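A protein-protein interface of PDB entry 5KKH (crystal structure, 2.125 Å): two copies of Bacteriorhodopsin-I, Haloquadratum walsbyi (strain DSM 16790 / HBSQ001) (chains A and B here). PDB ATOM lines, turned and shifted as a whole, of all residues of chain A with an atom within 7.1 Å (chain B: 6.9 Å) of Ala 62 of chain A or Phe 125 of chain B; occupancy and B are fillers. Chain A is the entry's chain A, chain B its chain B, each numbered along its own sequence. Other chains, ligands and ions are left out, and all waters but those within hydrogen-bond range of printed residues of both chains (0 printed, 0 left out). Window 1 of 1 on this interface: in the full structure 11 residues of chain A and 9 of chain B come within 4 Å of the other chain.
Ala 58 of chain A touches Phe 125 of chain B. Ile 59 of chain A touches Phe 125 of chain B. CB of Ala 62 of chain A touches CE1 of Phe 125 of chain B (3.9 Å). Ala 62 of chain A touches Phe 145 of chain B. Leu 65 of chain A touches Phe 145 of chain B (CB to CZ, 3.9 Å). Phe 145 of chain B touches Ser 66 of chain A.
Printed residues of chain B that touch a printed residue of chain A: Phe 125 and Phe 145. Of the 19 printed residues of chain A, 5 touch a printed residue of chain B. Hydrophobic or aromatic side chains of chain A that line the printed part of chain B: Ala 62 and Leu 65. Among the printed residues, 6 pairs touch across the chains.
OG1 of Thr 24 of chain A is in hydrogen-bond range of N of Leu 65 of chain A, 3.3 Å away. The backbone carbonyl oxygen (O) of Ile 59 of chain A is in hydrogen-bond range of the side-chain hydroxyl (OG) of Ser 63 of chain A. O of Ser 63 of chain A is in hydrogen-bond range of OG of Ser 66 of chain A (2.8 Å). The backbone carbonyl oxygen (O) of Phe 125 of chain B lies within hydrogen-bond range of the side-chain hydroxyl (OG1) of Thr 129 of chain B (2.7 Å).
No position is printed for both chains. Of the 6 pairs that touch across the chains among the printed residues, none has its exchanged pair printed and touching as well.
Printed residues of chain B within 4 Å of Ala 62 of chain A: Phe 125 (3.9 Å) and Phe 145 (3.4 Å). Of the printed residues of chain B, Leu 65 of chain A touches Phe 145 (3.9 Å). Val 120 of chain B touches none of the printed residues of chain A. Ile 127 of chain B touches none of the printed residues of chain A. Printed residues of chain A within 4 Å of Phe 145 of chain B: Ala 62, Leu 65 and Ser 66. The nearest residue of chain A that does not touch Phe 125 of chain B is Leu 55 of chain A (4.5 Å).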
ATOM      1  N   THR A  24      26.304  28.738  25.772  1.00  0.00           N
ATOM      2  CA  THR A  24      26.810  27.653  24.928  1.00  0.00           C
ATOM      3  C   THR A  24      28.257  27.912  24.494  1.00  0.00           C
ATOM      4  O   THR A  24      29.135  27.056  24.682  1.00  0.00           O
ATOM      5  CB  THR A  24      25.903  27.472  23.708  1.00  0.00           C
ATOM      6  OG1 THR A  24      24.544  27.320  24.131  1.00  0.00           O
ATOM      7  CG2 THR A  24      26.310  26.261  22.896  1.00  0.00           C
ATOM      8  N   MET A  27      30.870  28.031  27.512  1.00  0.00           N
ATOM      9  CA  MET A  27      31.190  26.691  27.990  1.00  0.00           C
ATOM     10  C   MET A  27      32.080  25.956  26.997  1.00  0.00           C
ATOM     11  O   MET A  27      33.046  25.290  27.385  1.00  0.00           O
ATOM     12  CB  MET A  27      29.908  25.896  28.229  1.00  0.00           C
ATOM     13  CG  MET A  27      29.033  26.471  29.349  1.00  0.00           C
ATOM     14  SD  MET A  27      29.871  26.406  30.934  1.00  0.00           S
ATOM     15  CE  MET A  27      28.643  27.175  32.014  1.00  0.00           C
ATOM     16  N   MET A  31      35.715  24.471  27.805  1.00  0.00           N
ATOM     17  CA  MET A  31      36.009  23.058  27.579  1.00  0.00           C
ATOM     18  C   MET A  31      37.191  22.896  26.628  1.00  0.00           C
ATOM     19  O   MET A  31      38.074  22.048  26.851  1.00  0.00           O
ATOM     20  CB  MET A  31      34.763  22.346  27.027  1.00  0.00           C
ATOM     21  CG  MET A  31      34.994  20.897  26.604  1.00  0.00           C
ATOM     22  SD  MET A  31      33.666  20.207  25.602  1.00  0.00           S
ATOM     23  CE  MET A  31      34.280  20.615  23.965  1.00  0.00           C
ATOM     24  N   LEU A  55      34.566  17.576  31.390  1.00  0.00           N
ATOM     25  CA  LEU A  55      33.208  17.055  31.286  1.00  0.00           C
ATOM     26  C   LEU A  55      32.178  18.070  31.764  1.00  0.00           C
ATOM     27  O   LEU A  55      31.107  18.208  31.167  1.00  0.00           O
ATOM     28  CB  LEU A  55      33.108  15.772  32.103  1.00  0.00           C
ATOM     29  CG  LEU A  55      31.804  15.002  32.024  1.00  0.00           C
ATOM     30  CD1 LEU A  55      31.559  14.555  30.594  1.00  0.00           C
ATOM     31  CD2 LEU A  55      31.913  13.825  32.943  1.00  0.00           C
ATOM     32  N   ILE A  56      32.493  18.803  32.826  1.00  0.00           N
ATOM     33  CA  ILE A  56      31.560  19.767  33.412  1.00  0.00           C
ATOM     34  C   ILE A  56      31.104  20.779  32.361  1.00  0.00           C
ATOM     35  O   ILE A  56      29.897  20.861  32.068  1.00  0.00           O
ATOM     36  CB  ILE A  56      32.176  20.450  34.646  1.00  0.00           C
ATOM     37  CG1 ILE A  56      32.290  19.451  35.803  1.00  0.00           C
ATOM     38  CG2 ILE A  56      31.365  21.709  35.018  1.00  0.00           C
ATOM     39  CD1 ILE A  56      33.173  19.888  36.917  1.00  0.00           C
ATOM     40  N   PRO A  57      31.991  21.561  31.742  1.00  0.00           N
ATOM     41  CA  PRO A  57      31.497  22.509  30.736  1.00  0.00           C
ATOM     42  C   PRO A  57      31.007  21.816  29.477  1.00  0.00           C
ATOM     43  O   PRO A  57      30.234  22.420  28.728  1.00  0.00           O
ATOM     44  CB  PRO A  57      32.708  23.409  30.471  1.00  0.00           C
ATOM     45  CG  PRO A  57      33.879  22.494  30.707  1.00  0.00           C
ATOM     46  CD  PRO A  57      33.459  21.652  31.884  1.00  0.00           C
ATOM     47  N   ALA A  58      31.415  20.564  29.227  1.00  0.00           N
ATOM     48  CA  ALA A  58      30.790  19.792  28.155  1.00  0.00           C
ATOM     49  C   ALA A  58      29.303  19.594  28.435  1.00  0.00           C
ATOM     50  O   ALA A  58      28.441  19.929  27.605  1.00  0.00           O
ATOM     51  CB  ALA A  58      31.494  18.449  27.999  1.00  0.00           C
ATOM     52  N   ILE A  59      28.984  19.068  29.618  1.00  0.00           N
ATOM     53  CA  ILE A  59      27.584  18.910  29.998  1.00  0.00           C
ATOM     54  C   ILE A  59      26.844  20.238  29.860  1.00  0.00           C
ATOM     55  O   ILE A  59      25.791  20.321  29.209  1.00  0.00           O
ATOM     56  CB  ILE A  59      27.494  18.326  31.415  1.00  0.00           C
ATOM     57  CG1 ILE A  59      28.129  16.920  31.399  1.00  0.00           C
ATOM     58  CG2 ILE A  59      26.081  18.246  31.857  1.00  0.00           C
ATOM     59  CD1 ILE A  59      28.391  16.329  32.741  1.00  0.00           C
ATOM     60  N   ALA A  60      27.416  21.307  30.418  1.00  0.00           N
ATOM     61  CA  ALA A  60      26.716  22.593  30.416  1.00  0.00           C
ATOM     62  C   ALA A  60      26.557  23.132  29.002  1.00  0.00           C
ATOM     63  O   ALA A  60      25.491  23.648  28.645  1.00  0.00           O
ATOM     64  CB  ALA A  60      27.452  23.607  31.287  1.00  0.00           C
ATOM     65  N   ALA A  61      27.594  22.999  28.177  1.00  0.00           N
ATOM     66  CA  ALA A  61      27.469  23.447  26.798  1.00  0.00           C
ATOM     67  C   ALA A  61      26.298  22.741  26.124  1.00  0.00           C
ATOM     68  O   ALA A  61      25.425  23.384  25.537  1.00  0.00           O
ATOM     69  CB  ALA A  61      28.774  23.197  26.038  1.00  0.00           C
ATOM     70  N   ALA A  62      26.234  21.417  26.283  1.00  0.00           N
ATOM     71  CA  ALA A  62      25.161  20.619  25.711  1.00  0.00           C
ATOM     72  C   ALA A  62      23.798  21.083  26.204  1.00  0.00           C
ATOM     73  O   ALA A  62      22.883  21.280  25.400  1.00  0.00           O
ATOM     74  CB  ALA A  62      25.381  19.138  26.038  1.00  0.00           C
ATOM     75  N   SER A  63      23.642  21.277  27.526  1.00  0.00           N
ATOM     76  CA  SER A  63      22.337  21.703  28.038  1.00  0.00           C
ATOM     77  C   SER A  63      22.004  23.121  27.597  1.00  0.00           C
ATOM     78  O   SER A  63      20.846  23.418  27.262  1.00  0.00           O
ATOM     79  CB  SER A  63      22.282  21.607  29.556  1.00  0.00           C
ATOM     80  OG  SER A  63      23.358  22.296  30.145  1.00  0.00           O
ATOM     81  N   TYR A  64      23.004  24.009  27.588  1.00  0.00           N
ATOM     82  CA  TYR A  64      22.773  25.359  27.076  1.00  0.00           C
ATOM     83  C   TYR A  64      22.330  25.323  25.621  1.00  0.00           C
ATOM     84  O   TYR A  64      21.392  26.032  25.240  1.00  0.00           O
ATOM     85  CB  TYR A  64      24.026  26.228  27.270  1.00  0.00           C
ATOM     86  CG  TYR A  64      23.919  27.066  28.536  1.00  0.00           C
ATOM     87  CD1 TYR A  64      24.200  26.505  29.787  1.00  0.00           C
ATOM     88  CD2 TYR A  64      23.469  28.395  28.494  1.00  0.00           C
ATOM     89  CE1 TYR A  64      24.057  27.252  30.979  1.00  0.00           C
ATOM     90  CE2 TYR A  64      23.349  29.154  29.676  1.00  0.00           C
ATOM     91  CZ  TYR A  64      23.645  28.574  30.910  1.00  0.00           C
ATOM     92  OH  TYR A  64      23.525  29.292  32.083  1.00  0.00           O
ATOM     93  N   LEU A  65      22.951  24.465  24.801  1.00  0.00           N
ATOM     94  CA  LEU A  65      22.522  24.376  23.405  1.00  0.00           C
ATOM     95  C   LEU A  65      21.094  23.849  23.299  1.00  0.00           C
ATOM     96  O   LEU A  65      20.277  24.408  22.559  1.00  0.00           O
ATOM     97  CB  LEU A  65      23.470  23.495  22.604  1.00  0.00           C
ATOM     98  CG  LEU A  65      23.111  23.421  21.109  1.00  0.00           C
ATOM     99  CD1 LEU A  65      23.159  24.809  20.514  1.00  0.00           C
ATOM    100  CD2 LEU A  65      24.064  22.484  20.350  1.00  0.00           C
ATOM    101  N   SER A  66      20.763  22.796  24.057  1.00  0.00           N
ATOM    102  CA  SER A  66      19.400  22.270  24.024  1.00  0.00           C
ATOM    103  C   SER A  66      18.390  23.325  24.460  1.00  0.00           C
ATOM    104  O   SER A  66      17.274  23.376  23.937  1.00  0.00           O
ATOM    105  CB  SER A  66      19.286  21.028  24.909  1.00  0.00           C
ATOM    106  OG  SER A  66      19.142  21.391  26.276  1.00  0.00           O
ATOM    107  N   MET A  67      18.757  24.158  25.435  1.00  0.00           N
ATOM    108  CA  MET A  67      17.909  25.273  25.837  1.00  0.00           C
ATOM    109  C   MET A  67      17.841  26.337  24.751  1.00  0.00           C
ATOM    110  O   MET A  67      16.803  26.982  24.565  1.00  0.00           O
ATOM    111  CB  MET A  67      18.431  25.886  27.141  1.00  0.00           C
ATOM    112  CG  MET A  67      18.178  25.028  28.371  1.00  0.00           C
ATOM    113  SD  MET A  67      18.610  25.875  29.900  1.00  0.00           S
ATOM    114  CE  MET A  67      20.427  25.797  29.856  1.00  0.00           C
ATOM    115  N   PHE A  68      18.947  26.553  24.035  1.00  0.00           N
ATOM    116  CA  PHE A  68      18.899  27.473  22.908  1.00  0.00           C
ATOM    117  C   PHE A  68      17.888  27.008  21.866  1.00  0.00           C
ATOM    118  O   PHE A  68      17.141  27.816  21.297  1.00  0.00           O
ATOM    119  CB  PHE A  68      20.285  27.599  22.290  1.00  0.00           C
ATOM    120  CG  PHE A  68      20.334  28.523  21.110  1.00  0.00           C
ATOM    121  CD1 PHE A  68      20.195  29.895  21.278  1.00  0.00           C
ATOM    122  CD2 PHE A  68      20.537  28.024  19.835  1.00  0.00           C
ATOM    123  CE1 PHE A  68      20.247  30.747  20.196  1.00  0.00           C
ATOM    124  CE2 PHE A  68      20.616  28.868  18.761  1.00  0.00           C
ATOM    125  CZ  PHE A  68      20.468  30.227  18.933  1.00  0.00           C
ATOM    126  N   ALA A  89      15.866  22.072  31.628  1.00  0.00           N
ATOM    127  CA  ALA A  89      17.117  21.389  31.276  1.00  0.00           C
ATOM    128  C   ALA A  89      18.271  21.813  32.181  1.00  0.00           C
ATOM    129  O   ALA A  89      19.210  21.034  32.394  1.00  0.00           O
ATOM    130  CB  ALA A  89      17.479  21.646  29.810  1.00  0.00           C
ATOM    131  N   ASP A  93      21.426  19.512  33.840  1.00  0.00           N
ATOM    132  CA  ASP A  93      22.828  19.939  33.875  1.00  0.00           C
ATOM    133  C   ASP A  93      23.373  19.936  35.305  1.00  0.00           C
ATOM    134  O   ASP A  93      24.430  19.356  35.579  1.00  0.00           O
ATOM    135  CB  ASP A  93      22.933  21.332  33.221  1.00  0.00           C
ATOM    136  CG  ASP A  93      24.288  22.047  33.453  1.00  0.00           C
ATOM    137  OD1 ASP A  93      25.258  21.471  33.994  1.00  0.00           O
ATOM    138  OD2 ASP A  93      24.378  23.230  33.056  1.00  0.00           O
ATOM    139  N   LEU B  95      21.334   3.923  28.818  1.00  0.00           N
ATOM    140  CA  LEU B  95      21.934   4.740  29.871  1.00  0.00           C
ATOM    141  C   LEU B  95      22.595   3.878  30.940  1.00  0.00           C
ATOM    142  O   LEU B  95      23.593   4.285  31.537  1.00  0.00           O
ATOM    143  CB  LEU B  95      20.891   5.667  30.503  1.00  0.00           C
ATOM    144  CG  LEU B  95      21.468   6.649  31.532  1.00  0.00           C
ATOM    145  CD1 LEU B  95      22.492   7.536  30.867  1.00  0.00           C
ATOM    146  CD2 LEU B  95      20.391   7.495  32.215  1.00  0.00           C
ATOM    147  N   VAL B 120      32.960   5.927  31.463  1.00  0.00           N
ATOM    148  CA  VAL B 120      31.540   5.941  31.808  1.00  0.00           C
ATOM    149  C   VAL B 120      30.965   7.357  31.709  1.00  0.00           C
ATOM    150  O   VAL B 120      29.810   7.553  31.300  1.00  0.00           O
ATOM    151  CB  VAL B 120      31.352   5.337  33.212  1.00  0.00           C
ATOM    152  CG1 VAL B 120      29.985   5.693  33.793  1.00  0.00           C
ATOM    153  CG2 VAL B 120      31.539   3.815  33.130  1.00  0.00           C
ATOM    154  N   GLY B 121      31.762   8.365  32.067  1.00  0.00           N
ATOM    155  CA  GLY B 121      31.310   9.738  31.914  1.00  0.00           C
ATOM    156  C   GLY B 121      31.094  10.122  30.461  1.00  0.00           C
ATOM    157  O   GLY B 121      30.087  10.742  30.114  1.00  0.00           O
ATOM    158  N   ILE B 122      32.047   9.778  29.594  1.00  0.00           N
ATOM    159  CA  ILE B 122      31.871  10.091  28.177  1.00  0.00           C
ATOM    160  C   ILE B 122      30.696   9.307  27.603  1.00  0.00           C
ATOM    161  O   ILE B 122      29.891   9.844  26.832  1.00  0.00           O
ATOM    162  CB  ILE B 122      33.177   9.825  27.409  1.00  0.00           C
ATOM    163  CG1 ILE B 122      34.335  10.625  28.024  1.00  0.00           C
ATOM    164  CG2 ILE B 122      33.019  10.213  25.956  1.00  0.00           C
ATOM    165  CD1 ILE B 122      35.711  10.044  27.721  1.00  0.00           C
ATOM    166  N   ASP B 123      30.551   8.043  28.013  1.00  0.00           N
ATOM    167  CA  ASP B 123      29.429   7.215  27.578  1.00  0.00           C
ATOM    168  C   ASP B 123      28.086   7.832  27.929  1.00  0.00           C
ATOM    169  O   ASP B 123      27.173   7.872  27.094  1.00  0.00           O
ATOM    170  CB  ASP B 123      29.517   5.848  28.217  1.00  0.00           C
ATOM    171  CG  ASP B 123      28.382   4.957  27.798  1.00  0.00           C
ATOM    172  OD1 ASP B 123      27.343   4.938  28.487  1.00  0.00           O
ATOM    173  OD2 ASP B 123      28.540   4.272  26.767  1.00  0.00           O
ATOM    174  N   ALA B 124      27.923   8.261  29.188  1.00  0.00           N
ATOM    175  CA  ALA B 124      26.659   8.854  29.613  1.00  0.00           C
ATOM    176  C   ALA B 124      26.337  10.088  28.782  1.00  0.00           C
ATOM    177  O   ALA B 124      25.214  10.244  28.283  1.00  0.00           O
ATOM    178  CB  ALA B 124      26.722   9.204  31.103  1.00  0.00           C
ATOM    179  N   PHE B 125      27.331  10.965  28.613  1.00  0.00           N
ATOM    180  CA  PHE B 125      27.208  12.118  27.726  1.00  0.00           C
ATOM    181  C   PHE B 125      26.762  11.683  26.340  1.00  0.00           C
ATOM    182  O   PHE B 125      25.857  12.280  25.750  1.00  0.00           O
ATOM    183  CB  PHE B 125      28.551  12.848  27.649  1.00  0.00           C
ATOM    184  CG  PHE B 125      28.505  14.170  26.912  1.00  0.00           C
ATOM    185  CD1 PHE B 125      28.115  15.322  27.559  1.00  0.00           C
ATOM    186  CD2 PHE B 125      28.879  14.247  25.585  1.00  0.00           C
ATOM    187  CE1 PHE B 125      28.103  16.550  26.899  1.00  0.00           C
ATOM    188  CE2 PHE B 125      28.877  15.468  24.912  1.00  0.00           C
ATOM    189  CZ  PHE B 125      28.482  16.627  25.570  1.00  0.00           C
ATOM    190  N   MET B 126      27.375  10.618  25.817  1.00  0.00           N
ATOM    191  CA  MET B 126      26.992  10.109  24.504  1.00  0.00           C
ATOM    192  C   MET B 126      25.494   9.775  24.454  1.00  0.00           C
ATOM    193  O   MET B 126      24.763  10.240  23.563  1.00  0.00           O
ATOM    194  CB  MET B 126      27.856   8.885  24.176  1.00  0.00           C
ATOM    195  CG  MET B 126      27.672   8.339  22.776  1.00  0.00           C
ATOM    196  SD  MET B 126      28.484   6.759  22.519  1.00  0.00           S
ATOM    197  CE  MET B 126      27.724   5.799  23.846  1.00  0.00           C
ATOM    198  N   ILE B 127      25.019   8.991  25.427  1.00  0.00           N
ATOM    199  CA  ILE B 127      23.643   8.500  25.411  1.00  0.00           C
ATOM    200  C   ILE B 127      22.657   9.645  25.594  1.00  0.00           C
ATOM    201  O   ILE B 127      21.659   9.730  24.884  1.00  0.00           O
ATOM    202  CB  ILE B 127      23.443   7.425  26.498  1.00  0.00           C
ATOM    203  CG1 ILE B 127      24.390   6.233  26.287  1.00  0.00           C
ATOM    204  CG2 ILE B 127      21.993   6.990  26.540  1.00  0.00           C
ATOM    205  CD1 ILE B 127      24.243   5.466  24.944  1.00  0.00           C
ATOM    206  N   VAL B 128      22.908  10.534  26.561  1.00  0.00           N
ATOM    207  CA  VAL B 128      21.930  11.580  26.857  1.00  0.00           C
ATOM    208  C   VAL B 128      21.842  12.582  25.706  1.00  0.00           C
ATOM    209  O   VAL B 128      20.743  13.035  25.351  1.00  0.00           O
ATOM    210  CB  VAL B 128      22.262  12.274  28.197  1.00  0.00           C
ATOM    211  CG1 VAL B 128      21.299  13.433  28.462  1.00  0.00           C
ATOM    212  CG2 VAL B 128      22.209  11.259  29.346  1.00  0.00           C
ATOM    213  N   THR B 129      22.988  12.944  25.105  1.00  0.00           N
ATOM    214  CA  THR B 129      22.939  13.803  23.922  1.00  0.00           C
ATOM    215  C   THR B 129      22.227  13.098  22.785  1.00  0.00           C
ATOM    216  O   THR B 129      21.561  13.752  21.981  1.00  0.00           O
ATOM    217  CB  THR B 129      24.340  14.258  23.476  1.00  0.00           C
ATOM    218  OG1 THR B 129      25.190  13.139  23.230  1.00  0.00           O
ATOM    219  CG2 THR B 129      24.997  15.177  24.520  1.00  0.00           C
ATOM    220  N   GLY B 130      22.328  11.764  22.718  1.00  0.00           N
ATOM    221  CA  GLY B 130      21.532  11.022  21.752  1.00  0.00           C
ATOM    222  C   GLY B 130      20.048  11.110  22.058  1.00  0.00           C
ATOM    223  O   GLY B 130      19.233  11.257  21.154  1.00  0.00           O
ATOM    224  N   LEU B 131      19.686  11.055  23.345  1.00  0.00           N
ATOM    225  CA  LEU B 131      18.296  11.216  23.733  1.00  0.00           C
ATOM    226  C   LEU B 131      17.765  12.578  23.291  1.00  0.00           C
ATOM    227  O   LEU B 131      16.645  12.681  22.792  1.00  0.00           O
ATOM    228  CB  LEU B 131      18.160  11.051  25.250  1.00  0.00           C
ATOM    229  CG  LEU B 131      16.721  11.035  25.774  1.00  0.00           C
ATOM    230  CD1 LEU B 131      15.861  10.014  25.003  1.00  0.00           C
ATOM    231  CD2 LEU B 131      16.653  10.757  27.264  1.00  0.00           C
ATOM    232  N   VAL B 132      18.565  13.631  23.448  1.00  0.00           N
ATOM    233  CA  VAL B 132      18.106  14.963  23.068  1.00  0.00           C
ATOM    234  C   VAL B 132      17.869  15.029  21.572  1.00  0.00           C
ATOM    235  O   VAL B 132      16.832  15.529  21.119  1.00  0.00           O
ATOM    236  CB  VAL B 132      19.113  16.030  23.531  1.00  0.00           C
ATOM    237  CG1 VAL B 132      18.858  17.326  22.844  1.00  0.00           C
ATOM    238  CG2 VAL B 132      19.002  16.215  25.045  1.00  0.00           C
ATOM    239  N   PHE B 145      22.669  17.471  17.794  1.00  0.00           N
ATOM    240  CA  PHE B 145      22.948  16.576  18.909  1.00  0.00           C
ATOM    241  C   PHE B 145      23.353  15.188  18.442  1.00  0.00           C
ATOM    242  O   PHE B 145      24.164  14.548  19.113  1.00  0.00           O
ATOM    243  CB  PHE B 145      21.788  16.535  19.904  1.00  0.00           C
ATOM    244  CG  PHE B 145      21.762  17.744  20.810  1.00  0.00           C
ATOM    245  CD1 PHE B 145      22.444  17.736  22.020  1.00  0.00           C
ATOM    246  CD2 PHE B 145      21.105  18.911  20.416  1.00  0.00           C
ATOM    247  CE1 PHE B 145      22.442  18.864  22.842  1.00  0.00           C
ATOM    248  CE2 PHE B 145      21.091  20.046  21.241  1.00  0.00           C
ATOM    249  CZ  PHE B 145      21.757  20.025  22.450  1.00  0.00           C
ATOM    250  N   ILE B 148      27.130  15.870  18.111  1.00  0.00           N
ATOM    251  CA  ILE B 148      27.822  15.872  19.407  1.00  0.00           C
ATOM    252  C   ILE B 148      27.908  14.459  19.988  1.00  0.00           C
ATOM    253  O   ILE B 148      28.939  14.058  20.554  1.00  0.00           O
ATOM    254  CB  ILE B 148      27.160  16.851  20.396  1.00  0.00           C
ATOM    255  CG1 ILE B 148      27.708  16.669  21.802  1.00  0.00           C
ATOM    256  CG2 ILE B 148      25.734  16.578  20.570  1.00  0.00           C
ATOM    257  CD1 ILE B 148      29.198  16.990  21.917  1.00  0.00           C
ATOM    258  N   SER B 149      26.844  13.678  19.863  1.00  0.00           N
ATOM    259  CA  SER B 149      26.878  12.331  20.435  1.00  0.00           C
ATOM    260  C   SER B 149      27.862  11.434  19.682  1.00  0.00           C
ATOM    261  O   SER B 149      28.645  10.698  20.299  1.00  0.00           O
ATOM    262  CB  SER B 149      25.461  11.735  20.452  1.00  0.00           C
ATOM    263  OG  SER B 149      25.468  10.415  21.008  1.00  0.00           O
ATOM    264  N   SER B 152      31.270  12.300  20.685  1.00  0.00           N
ATOM    265  CA  SER B 152      31.600  11.663  21.951  1.00  0.00           C
ATOM    266  C   SER B 152      31.853  10.172  21.770  1.00  0.00           C
ATOM    267  O   SER B 152      32.702   9.608  22.460  1.00  0.00           O
ATOM    268  CB  SER B 152      30.501  11.917  22.987  1.00  0.00           C
ATOM    269  OG  SER B 152      29.248  11.428  22.563  1.00  0.00           O
ATOM    270  N   PHE B 155      35.497   9.680  20.697  1.00  0.00           N
ATOM    271  CA  PHE B 155      36.381   9.706  21.855  1.00  0.00           C
ATOM    272  C   PHE B 155      36.324   8.379  22.585  1.00  0.00           C
ATOM    273  O   PHE B 155      37.320   7.665  22.680  1.00  0.00           O
ATOM    274  CB  PHE B 155      35.996  10.808  22.832  1.00  0.00           C
ATOM    275  CG  PHE B 155      35.891  12.147  22.234  1.00  0.00           C
ATOM    276  CD1 PHE B 155      36.910  12.661  21.470  1.00  0.00           C
ATOM    277  CD2 PHE B 155      34.773  12.910  22.453  1.00  0.00           C
ATOM    278  CE1 PHE B 155      36.798  13.925  20.920  1.00  0.00           C
ATOM    279  CE2 PHE B 155      34.666  14.168  21.904  1.00  0.00           C
ATOM    280  CZ  PHE B 155      35.683  14.670  21.146  1.00  0.00           C
